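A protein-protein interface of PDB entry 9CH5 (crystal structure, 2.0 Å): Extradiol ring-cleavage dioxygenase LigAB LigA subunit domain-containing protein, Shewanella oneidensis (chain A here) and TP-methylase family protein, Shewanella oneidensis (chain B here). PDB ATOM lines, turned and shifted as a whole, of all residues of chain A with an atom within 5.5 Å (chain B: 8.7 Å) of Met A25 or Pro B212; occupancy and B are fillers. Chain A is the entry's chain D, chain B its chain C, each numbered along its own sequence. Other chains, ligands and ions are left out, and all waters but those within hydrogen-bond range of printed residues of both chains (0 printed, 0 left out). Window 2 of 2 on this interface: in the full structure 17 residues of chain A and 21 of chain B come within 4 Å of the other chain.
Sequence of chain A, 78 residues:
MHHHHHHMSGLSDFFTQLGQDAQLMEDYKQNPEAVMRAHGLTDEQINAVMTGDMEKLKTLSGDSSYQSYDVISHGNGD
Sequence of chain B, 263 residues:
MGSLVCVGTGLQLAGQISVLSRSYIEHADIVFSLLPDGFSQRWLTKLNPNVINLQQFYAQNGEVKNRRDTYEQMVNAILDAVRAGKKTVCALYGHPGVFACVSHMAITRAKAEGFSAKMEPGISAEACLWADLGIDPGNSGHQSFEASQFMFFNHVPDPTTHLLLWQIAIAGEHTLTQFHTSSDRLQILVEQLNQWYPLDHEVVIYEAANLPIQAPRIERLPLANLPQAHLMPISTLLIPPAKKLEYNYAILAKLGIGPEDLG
Of the printed residues of chain B, Phe A15 touches Leu B13 (3.5 Å), Phe B39 (3.7 Å), Pro B212 (3.5 Å) and Ile B213 (3.5 Å).
Met A25 touches one residue of chain B.
Glu A26 touches none of the printed residues of chain B.
Of the printed residues of chain A, Leu B13 touches Phe A15 (3.5 Å) and Gly A19 (3.7 Å).
Of the printed residues of chain A, Gly B15 touches Gly A19 (3.3 Å).
Of the printed residues of chain A, Phe B39 touches Phe A15 (3.7 Å).
Of chain A, only Phe A15, Leu A18, Gly A19 and Met A25 come within 4 Å of Pro B212.
Of the printed residues of chain A, Ile B213 touches Phe A15 (3.5 Å), Leu A18 (3.7 Å) and Tyr A28 (3.2 Å).
The nearest residue of chain B that does not touch Met A25 is Ile B213 (6.2 Å).
Of the 15 printed residues of chain B, 5 touch a printed residue of chain A.
Printed residues of chain B that touch a printed residue of chain A: Leu B13, Gly B15, Phe B39, Pro B212 and Ile B213.
Hydrophobic or aromatic side chains of chain B that line the printed part of chain A: Leu B13, Phe B39, Pro B212 and Ile B213.
Along chain B the printed residues that touch a printed residue of chain A span positions 13 to 213.
Of the 13 printed residues of chain A, 5 touch a printed residue of chain B.
Hydrophobic or aromatic side chains of chain A that line the printed part of chain B: Phe A15, Leu A18, Met A25 and Tyr A28.
Among the printed residues, 11 pairs touch across the chains.
Among the printed residues, no Asp or Glu carboxylate lies within 4 Å of a Lys or Arg side-chain nitrogen of the other chain.
N of Leu B13 lies within hydrogen-bond range of O of Asn B210 (3.0 Å).
OD1 of Asp B37 is in hydrogen-bond range of N of Phe B39 (3.0 Å).
Among the printed residues, pairs that only touch across the chains: Tyr A28 with Ile B213 (3.2 Å), Gly A19 with Gly B15 (3.3 Å), Phe A15 with Pro B212 (3.5 Å), Phe A15 with Ile B213 (3.5 Å), Phe A15 with Leu B13 (3.5 Å), Leu A18 with Ile B213 (3.7 Å), Phe A15 with Phe B39 (3.7 Å), Leu A18 with Pro B212 (3.7 Å), Gly A19 with Leu B13 (3.7 Å), Met A25 with Pro B212 (3.8 Å) and Gly A19 with Pro B212 (3.9 Å).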
ATOM      1  N   PHE A  15      28.727 -12.412 -16.156  1.00  0.00           N
ATOM      2  CA  PHE A  15      27.510 -11.611 -16.255  1.00  0.00           C
ATOM      3  C   PHE A  15      27.519 -10.753 -17.514  1.00  0.00           C
ATOM      4  O   PHE A  15      26.473 -10.555 -18.145  1.00  0.00           O
ATOM      5  CB  PHE A  15      27.351 -10.726 -15.016  1.00  0.00           C
ATOM      6  CG  PHE A  15      26.968 -11.472 -13.767  1.00  0.00           C
ATOM      7  CD1 PHE A  15      26.506 -12.778 -13.824  1.00  0.00           C
ATOM      8  CD2 PHE A  15      27.048 -10.850 -12.531  1.00  0.00           C
ATOM      9  CE1 PHE A  15      26.149 -13.452 -12.669  1.00  0.00           C
ATOM     10  CE2 PHE A  15      26.691 -11.519 -11.374  1.00  0.00           C
ATOM     11  CZ  PHE A  15      26.241 -12.820 -11.444  1.00  0.00           C
ATOM     12  N   LEU A  18      26.759 -13.044 -20.404  1.00  0.00           N
ATOM     13  CA  LEU A  18      25.381 -13.519 -20.338  1.00  0.00           C
ATOM     14  C   LEU A  18      24.404 -12.433 -20.771  1.00  0.00           C
ATOM     15  O   LEU A  18      23.411 -12.716 -21.450  1.00  0.00           O
ATOM     16  CB  LEU A  18      25.078 -13.994 -18.915  1.00  0.00           C
ATOM     17  CG  LEU A  18      23.671 -14.477 -18.565  1.00  0.00           C
ATOM     18  CD1 LEU A  18      23.166 -15.455 -19.605  1.00  0.00           C
ATOM     19  CD2 LEU A  18      23.666 -15.118 -17.185  1.00  0.00           C
ATOM     20  N   GLY A  19      24.667 -11.182 -20.385  1.00  0.00           N
ATOM     21  CA  GLY A  19      23.778 -10.092 -20.744  1.00  0.00           C
ATOM     22  C   GLY A  19      23.786  -9.747 -22.218  1.00  0.00           C
ATOM     23  O   GLY A  19      22.809  -9.177 -22.715  1.00  0.00           O
ATOM     24  N   ASP A  21      24.834 -12.072 -24.863  1.00  0.00           N
ATOM     25  CA  ASP A  21      24.918 -13.213 -25.763  1.00  0.00           C
ATOM     26  C   ASP A  21      23.631 -14.021 -25.651  1.00  0.00           C
ATOM     27  O   ASP A  21      23.408 -14.723 -24.656  1.00  0.00           O
ATOM     28  CB  ASP A  21      26.151 -14.058 -25.428  1.00  0.00           C
ATOM     29  CG  ASP A  21      26.339 -15.245 -26.362  1.00  0.00           C
ATOM     30  OD1 ASP A  21      25.439 -15.553 -27.164  1.00  0.00           O
ATOM     31  OD2 ASP A  21      27.418 -15.872 -26.289  1.00  0.00           O
ATOM     32  N   ALA A  22      22.793 -13.927 -26.684  1.00  0.00           N
ATOM     33  CA  ALA A  22      21.520 -14.621 -26.634  1.00  0.00           C
ATOM     34  C   ALA A  22      21.713 -16.126 -26.750  1.00  0.00           C
ATOM     35  O   ALA A  22      20.829 -16.880 -26.310  1.00  0.00           O
ATOM     36  CB  ALA A  22      20.572 -14.104 -27.711  1.00  0.00           C
ATOM     37  N   GLN A  23      22.840 -16.598 -27.322  1.00  0.00           N
ATOM     38  CA  GLN A  23      23.071 -18.034 -27.228  1.00  0.00           C
ATOM     39  C   GLN A  23      23.131 -18.423 -25.762  1.00  0.00           C
ATOM     40  O   GLN A  23      22.366 -19.264 -25.274  1.00  0.00           O
ATOM     41  CB  GLN A  23      24.432 -18.500 -27.766  1.00  0.00           C
ATOM     42  CG  GLN A  23      24.346 -19.997 -27.569  1.00  0.00           C
ATOM     43  CD  GLN A  23      23.592 -20.662 -28.688  1.00  0.00           C
ATOM     44  OE1 GLN A  23      22.339 -20.897 -28.520  1.00  0.00           O
ATOM     45  NE2 GLN A  23      24.334 -21.482 -29.414  1.00  0.00           N
ATOM     46  N   LEU A  24      24.082 -17.814 -25.053  1.00  0.00           N
ATOM     47  CA  LEU A  24      24.348 -18.155 -23.668  1.00  0.00           C
ATOM     48  C   LEU A  24      23.121 -17.921 -22.810  1.00  0.00           C
ATOM     49  O   LEU A  24      22.830 -18.710 -21.902  1.00  0.00           O
ATOM     50  CB  LEU A  24      25.541 -17.333 -23.185  1.00  0.00           C
ATOM     51  CG  LEU A  24      25.878 -17.401 -21.706  1.00  0.00           C
ATOM     52  CD1 LEU A  24      26.066 -18.836 -21.229  1.00  0.00           C
ATOM     53  CD2 LEU A  24      27.112 -16.568 -21.390  1.00  0.00           C
ATOM     54  N   MET A  25      22.386 -16.844 -23.087  1.00  0.00           N
ATOM     55  CA  MET A  25      21.192 -16.551 -22.308  1.00  0.00           C
ATOM     56  C   MET A  25      20.197 -17.700 -22.369  1.00  0.00           C
ATOM     57  O   MET A  25      19.644 -18.102 -21.340  1.00  0.00           O
ATOM     58  CB  MET A  25      20.549 -15.260 -22.792  1.00  0.00           C
ATOM     59  CG  MET A  25      19.280 -14.921 -22.036  1.00  0.00           C
ATOM     60  SD  MET A  25      19.610 -14.663 -20.281  1.00  0.00           S
ATOM     61  CE  MET A  25      20.233 -12.983 -20.313  1.00  0.00           C
ATOM     62  N   GLU A  26      19.966 -18.252 -23.564  1.00  0.00           N
ATOM     63  CA  GLU A  26      19.030 -19.364 -23.673  1.00  0.00           C
ATOM     64  C   GLU A  26      19.633 -20.639 -23.099  1.00  0.00           C
ATOM     65  O   GLU A  26      18.901 -21.489 -22.574  1.00  0.00           O
ATOM     66  CB  GLU A  26      18.609 -19.555 -25.127  1.00  0.00           C
ATOM     67  CG  GLU A  26      17.603 -18.515 -25.615  1.00  0.00           C
ATOM     68  CD  GLU A  26      16.395 -18.392 -24.702  1.00  0.00           C
ATOM     69  OE1 GLU A  26      15.574 -19.332 -24.674  1.00  0.00           O
ATOM     70  OE2 GLU A  26      16.264 -17.355 -24.013  1.00  0.00           O
ATOM     71  N   ASP A  27      20.958 -20.789 -23.188  1.00  0.00           N
ATOM     72  CA  ASP A  27      21.628 -21.881 -22.485  1.00  0.00           C
ATOM     73  C   ASP A  27      21.396 -21.771 -20.985  1.00  0.00           C
ATOM     74  O   ASP A  27      21.074 -22.759 -20.313  1.00  0.00           O
ATOM     75  CB  ASP A  27      23.128 -21.868 -22.786  1.00  0.00           C
ATOM     76  CG  ASP A  27      23.444 -22.224 -24.221  1.00  0.00           C
ATOM     77  OD1 ASP A  27      22.549 -22.739 -24.925  1.00  0.00           O
ATOM     78  OD2 ASP A  27      24.597 -21.999 -24.645  1.00  0.00           O
ATOM     79  N   TYR A  28      21.560 -20.561 -20.442  1.00  0.00           N
ATOM     80  CA  TYR A  28      21.423 -20.356 -19.004  1.00  0.00           C
ATOM     81  C   TYR A  28      20.007 -20.656 -18.536  1.00  0.00           C
ATOM     82  O   TYR A  28      19.808 -21.285 -17.491  1.00  0.00           O
ATOM     83  CB  TYR A  28      21.814 -18.920 -18.645  1.00  0.00           C
ATOM     84  CG  TYR A  28      21.543 -18.530 -17.208  1.00  0.00           C
ATOM     85  CD1 TYR A  28      22.464 -18.807 -16.207  1.00  0.00           C
ATOM     86  CD2 TYR A  28      20.366 -17.879 -16.855  1.00  0.00           C
ATOM     87  CE1 TYR A  28      22.218 -18.452 -14.891  1.00  0.00           C
ATOM     88  CE2 TYR A  28      20.112 -17.524 -15.543  1.00  0.00           C
ATOM     89  CZ  TYR A  28      21.042 -17.813 -14.568  1.00  0.00           C
ATOM     90  OH  TYR A  28      20.793 -17.458 -13.260  1.00  0.00           O
ATOM     91  N   LYS A  29      19.006 -20.214 -19.297  1.00  0.00           N
ATOM     92  CA  LYS A  29      17.628 -20.411 -18.867  1.00  0.00           C
ATOM     93  C   LYS A  29      17.255 -21.889 -18.866  1.00  0.00           C
ATOM     94  O   LYS A  29      16.446 -22.323 -18.035  1.00  0.00           O
ATOM     95  CB  LYS A  29      16.690 -19.572 -19.731  1.00  0.00           C
ATOM     96  CG  LYS A  29      16.935 -18.081 -19.512  1.00  0.00           C
ATOM     97  CD  LYS A  29      15.660 -17.277 -19.386  1.00  0.00           C
ATOM     98  CE  LYS A  29      15.093 -16.903 -20.734  1.00  0.00           C
ATOM     99  NZ  LYS A  29      13.632 -16.683 -20.615  1.00  0.00           N
ATOM    100  N   GLN A  30      17.817 -22.668 -19.795  1.00  0.00           N
ATOM    101  CA  GLN A  30      17.574 -24.108 -19.811  1.00  0.00           C
ATOM    102  C   GLN A  30      18.065 -24.762 -18.525  1.00  0.00           C
ATOM    103  O   GLN A  30      17.353 -25.563 -17.907  1.00  0.00           O
ATOM    104  CB  GLN A  30      18.270 -24.738 -21.015  1.00  0.00           C
ATOM    105  CG  GLN A  30      17.670 -24.378 -22.361  1.00  0.00           C
ATOM    106  CD  GLN A  30      16.659 -25.396 -22.841  1.00  0.00           C
ATOM    107  OE1 GLN A  30      15.799 -25.845 -22.083  1.00  0.00           O
ATOM    108  NE2 GLN A  30      16.762 -25.775 -24.110  1.00  0.00           N
ATOM    109  N   LEU B  11      18.822  -0.650 -18.724  1.00  0.00           N
ATOM    110  CA  LEU B  11      18.792  -1.062 -17.326  1.00  0.00           C
ATOM    111  C   LEU B  11      19.605  -2.322 -17.080  1.00  0.00           C
ATOM    112  O   LEU B  11      20.251  -2.445 -16.035  1.00  0.00           O
ATOM    113  CB  LEU B  11      17.347  -1.282 -16.857  1.00  0.00           C
ATOM    114  CG  LEU B  11      16.515  -0.049 -16.464  1.00  0.00           C
ATOM    115  CD1 LEU B  11      17.041   0.558 -15.169  1.00  0.00           C
ATOM    116  CD2 LEU B  11      16.435   0.995 -17.569  1.00  0.00           C
ATOM    117  N   GLN B  12      19.595  -3.253 -18.029  1.00  0.00           N
ATOM    118  CA  GLN B  12      20.311  -4.508 -17.884  1.00  0.00           C
ATOM    119  C   GLN B  12      21.773  -4.350 -18.282  1.00  0.00           C
ATOM    120  O   GLN B  12      22.126  -3.549 -19.153  1.00  0.00           O
ATOM    121  CB  GLN B  12      19.660  -5.606 -18.726  1.00  0.00           C
ATOM    122  CG  GLN B  12      18.568  -6.375 -18.004  1.00  0.00           C
ATOM    123  CD  GLN B  12      19.122  -7.429 -17.065  1.00  0.00           C
ATOM    124  OE1 GLN B  12      20.335  -7.547 -16.896  1.00  0.00           O
ATOM    125  NE2 GLN B  12      18.235  -8.203 -16.451  1.00  0.00           N
ATOM    126  N   LEU B  13      22.620  -5.127 -17.618  1.00  0.00           N
ATOM    127  CA  LEU B  13      24.058  -5.123 -17.865  1.00  0.00           C
ATOM    128  C   LEU B  13      24.384  -5.418 -19.326  1.00  0.00           C
ATOM    129  O   LEU B  13      23.988  -6.460 -19.861  1.00  0.00           O
ATOM    130  CB  LEU B  13      24.721  -6.155 -16.952  1.00  0.00           C
ATOM    131  CG  LEU B  13      26.228  -6.363 -17.006  1.00  0.00           C
ATOM    132  CD1 LEU B  13      26.958  -5.072 -16.731  1.00  0.00           C
ATOM    133  CD2 LEU B  13      26.613  -7.415 -15.989  1.00  0.00           C
ATOM    134  N   ALA B  14      25.071  -4.469 -19.973  1.00  0.00           N
ATOM    135  CA  ALA B  14      25.840  -4.703 -21.194  1.00  0.00           C
ATOM    136  C   ALA B  14      24.983  -4.871 -22.445  1.00  0.00           C
ATOM    137  O   ALA B  14      25.339  -4.358 -23.511  1.00  0.00           O
ATOM    138  CB  ALA B  14      26.751  -5.926 -21.017  1.00  0.00           C
ATOM    139  N   GLY B  15      23.867  -5.590 -22.342  1.00  0.00           N
ATOM    140  CA  GLY B  15      23.144  -6.005 -23.529  1.00  0.00           C
ATOM    141  C   GLY B  15      21.995  -5.120 -23.964  1.00  0.00           C
ATOM    142  O   GLY B  15      21.476  -5.284 -25.070  1.00  0.00           O
ATOM    143  N   ASP B  37      25.507   0.028 -10.914  1.00  0.00           N
ATOM    144  CA  ASP B  37      26.274  -0.838 -10.028  1.00  0.00           C
ATOM    145  C   ASP B  37      27.705  -0.965 -10.536  1.00  0.00           C
ATOM    146  O   ASP B  37      28.098  -0.335 -11.522  1.00  0.00           O
ATOM    147  CB  ASP B  37      25.609  -2.213  -9.909  1.00  0.00           C
ATOM    148  CG  ASP B  37      25.376  -2.869 -11.259  1.00  0.00           C
ATOM    149  OD1 ASP B  37      26.344  -3.013 -12.041  1.00  0.00           O
ATOM    150  OD2 ASP B  37      24.220  -3.251 -11.545  1.00  0.00           O
ATOM    151  N   PHE B  39      29.184  -3.860 -11.565  1.00  0.00           N
ATOM    152  CA  PHE B  39      29.292  -4.726 -12.734  1.00  0.00           C
ATOM    153  C   PHE B  39      29.161  -3.905 -14.009  1.00  0.00           C
ATOM    154  O   PHE B  39      29.930  -4.080 -14.963  1.00  0.00           O
ATOM    155  CB  PHE B  39      28.213  -5.808 -12.701  1.00  0.00           C
ATOM    156  CG  PHE B  39      28.381  -6.816 -11.600  1.00  0.00           C
ATOM    157  CD1 PHE B  39      29.338  -7.815 -11.687  1.00  0.00           C
ATOM    158  CD2 PHE B  39      27.563  -6.777 -10.483  1.00  0.00           C
ATOM    159  CE1 PHE B  39      29.485  -8.746 -10.672  1.00  0.00           C
ATOM    160  CE2 PHE B  39      27.704  -7.703  -9.466  1.00  0.00           C
ATOM    161  CZ  PHE B  39      28.666  -8.688  -9.561  1.00  0.00           C
ATOM    162  N   ALA B 209      15.228  -5.443 -13.531  1.00  0.00           N
ATOM    163  CA  ALA B 209      16.479  -6.077 -13.140  1.00  0.00           C
ATOM    164  C   ALA B 209      17.670  -5.375 -13.780  1.00  0.00           C
ATOM    165  O   ALA B 209      17.596  -4.897 -14.914  1.00  0.00           O
ATOM    166  CB  ALA B 209      16.470  -7.555 -13.536  1.00  0.00           C
ATOM    167  N   ASN B 210      18.773  -5.308 -13.037  1.00  0.00           N
ATOM    168  CA  ASN B 210      20.015  -4.743 -13.548  1.00  0.00           C
ATOM    169  C   ASN B 210      21.016  -5.804 -13.986  1.00  0.00           C
ATOM    170  O   ASN B 210      21.953  -5.482 -14.724  1.00  0.00           O
ATOM    171  CB  ASN B 210      20.668  -3.841 -12.492  1.00  0.00           C
ATOM    172  CG  ASN B 210      19.884  -2.564 -12.249  1.00  0.00           C
ATOM    173  OD1 ASN B 210      19.472  -2.278 -11.123  1.00  0.00           O
ATOM    174  ND2 ASN B 210      19.668  -1.792 -13.306  1.00  0.00           N
ATOM    175  N   LEU B 211      20.837  -7.053 -13.558  1.00  0.00           N
ATOM    176  CA  LEU B 211      21.742  -8.142 -13.883  1.00  0.00           C
ATOM    177  C   LEU B 211      20.990  -9.262 -14.598  1.00  0.00           C
ATOM    178  O   LEU B 211      19.793  -9.458 -14.366  1.00  0.00           O
ATOM    179  CB  LEU B 211      22.411  -8.699 -12.619  1.00  0.00           C
ATOM    180  CG  LEU B 211      23.335  -7.726 -11.879  1.00  0.00           C
ATOM    181  CD1 LEU B 211      23.933  -8.381 -10.643  1.00  0.00           C
ATOM    182  CD2 LEU B 211      24.429  -7.215 -12.806  1.00  0.00           C
ATOM    183  N   PRO B 212      21.662 -10.013 -15.478  1.00  0.00           N
ATOM    184  CA  PRO B 212      20.951 -11.034 -16.266  1.00  0.00           C
ATOM    185  C   PRO B 212      20.546 -12.260 -15.467  1.00  0.00           C
ATOM    186  O   PRO B 212      19.772 -13.082 -15.983  1.00  0.00           O
ATOM    187  CB  PRO B 212      21.957 -11.390 -17.366  1.00  0.00           C
ATOM    188  CG  PRO B 212      23.291 -11.134 -16.747  1.00  0.00           C
ATOM    189  CD  PRO B 212      23.107  -9.999 -15.766  1.00  0.00           C
ATOM    190  N   ILE B 213      21.036 -12.415 -14.237  1.00  0.00           N
ATOM    191  CA  ILE B 213      20.647 -13.530 -13.381  1.00  0.00           C
ATOM    192  C   ILE B 213      19.564 -13.121 -12.393  1.00  0.00           C
ATOM    193  O   ILE B 213      19.230 -13.887 -11.485  1.00  0.00           O
ATOM    194  CB  ILE B 213      21.870 -14.126 -12.654  1.00  0.00           C
ATOM    195  CG1 ILE B 213      22.722 -13.052 -11.947  1.00  0.00           C
ATOM    196  CG2 ILE B 213      22.745 -14.893 -13.634  1.00  0.00           C
ATOM    197  CD1 ILE B 213      22.086 -12.333 -10.762  1.00  0.00           C
ATOM    198  N   GLN B 214      18.998 -11.933 -12.561  1.00  0.00           N
ATOM    199  CA  GLN B 214      18.128 -11.317 -11.573  1.00  0.00           C
ATOM    200  C   GLN B 214      16.718 -11.204 -12.129  1.00  0.00           C
ATOM    201  O   GLN B 214      16.525 -10.745 -13.259  1.00  0.00           O
ATOM    202  CB  GLN B 214      18.652  -9.932 -11.183  1.00  0.00           C
ATOM    203  CG  GLN B 214      17.675  -9.096 -10.373  1.00  0.00           C
ATOM    204  CD  GLN B 214      18.143  -7.665 -10.192  1.00  0.00           C
ATOM    205  OE1 GLN B 214      19.017  -7.189 -10.917  1.00  0.00           O
ATOM    206  NE2 GLN B 214      17.562  -6.972  -9.220  1.00  0.00           N
ATOM    207  N   ALA B 215      15.746 -11.628 -11.339  1.00  0.00           N
ATOM    208  CA  ALA B 215      14.355 -11.448 -11.701  1.00  0.00           C
ATOM    209  C   ALA B 215      13.906 -10.033 -11.338  1.00  0.00           C
ATOM    210  O   ALA B 215      14.410  -9.439 -10.382  1.00  0.00           O
ATOM    211  CB  ALA B 215      13.483 -12.470 -10.982  1.00  0.00           C
ATOM    212  N   PRO B 216      12.970  -9.464 -12.091  1.00  0.00           N
ATOM    213  CA  PRO B 216      12.444  -8.148 -11.729  1.00  0.00           C
ATOM    214  C   PRO B 216      11.606  -8.231 -10.466  1.00  0.00           C
ATOM    215  O   PRO B 216      11.085  -9.285 -10.099  1.00  0.00           O
ATOM    216  CB  PRO B 216      11.583  -7.770 -12.940  1.00  0.00           C
ATOM    217  CG  PRO B 216      11.110  -9.093 -13.452  1.00  0.00           C
ATOM    218  CD  PRO B 216      12.308  -9.999 -13.293  1.00  0.00           C
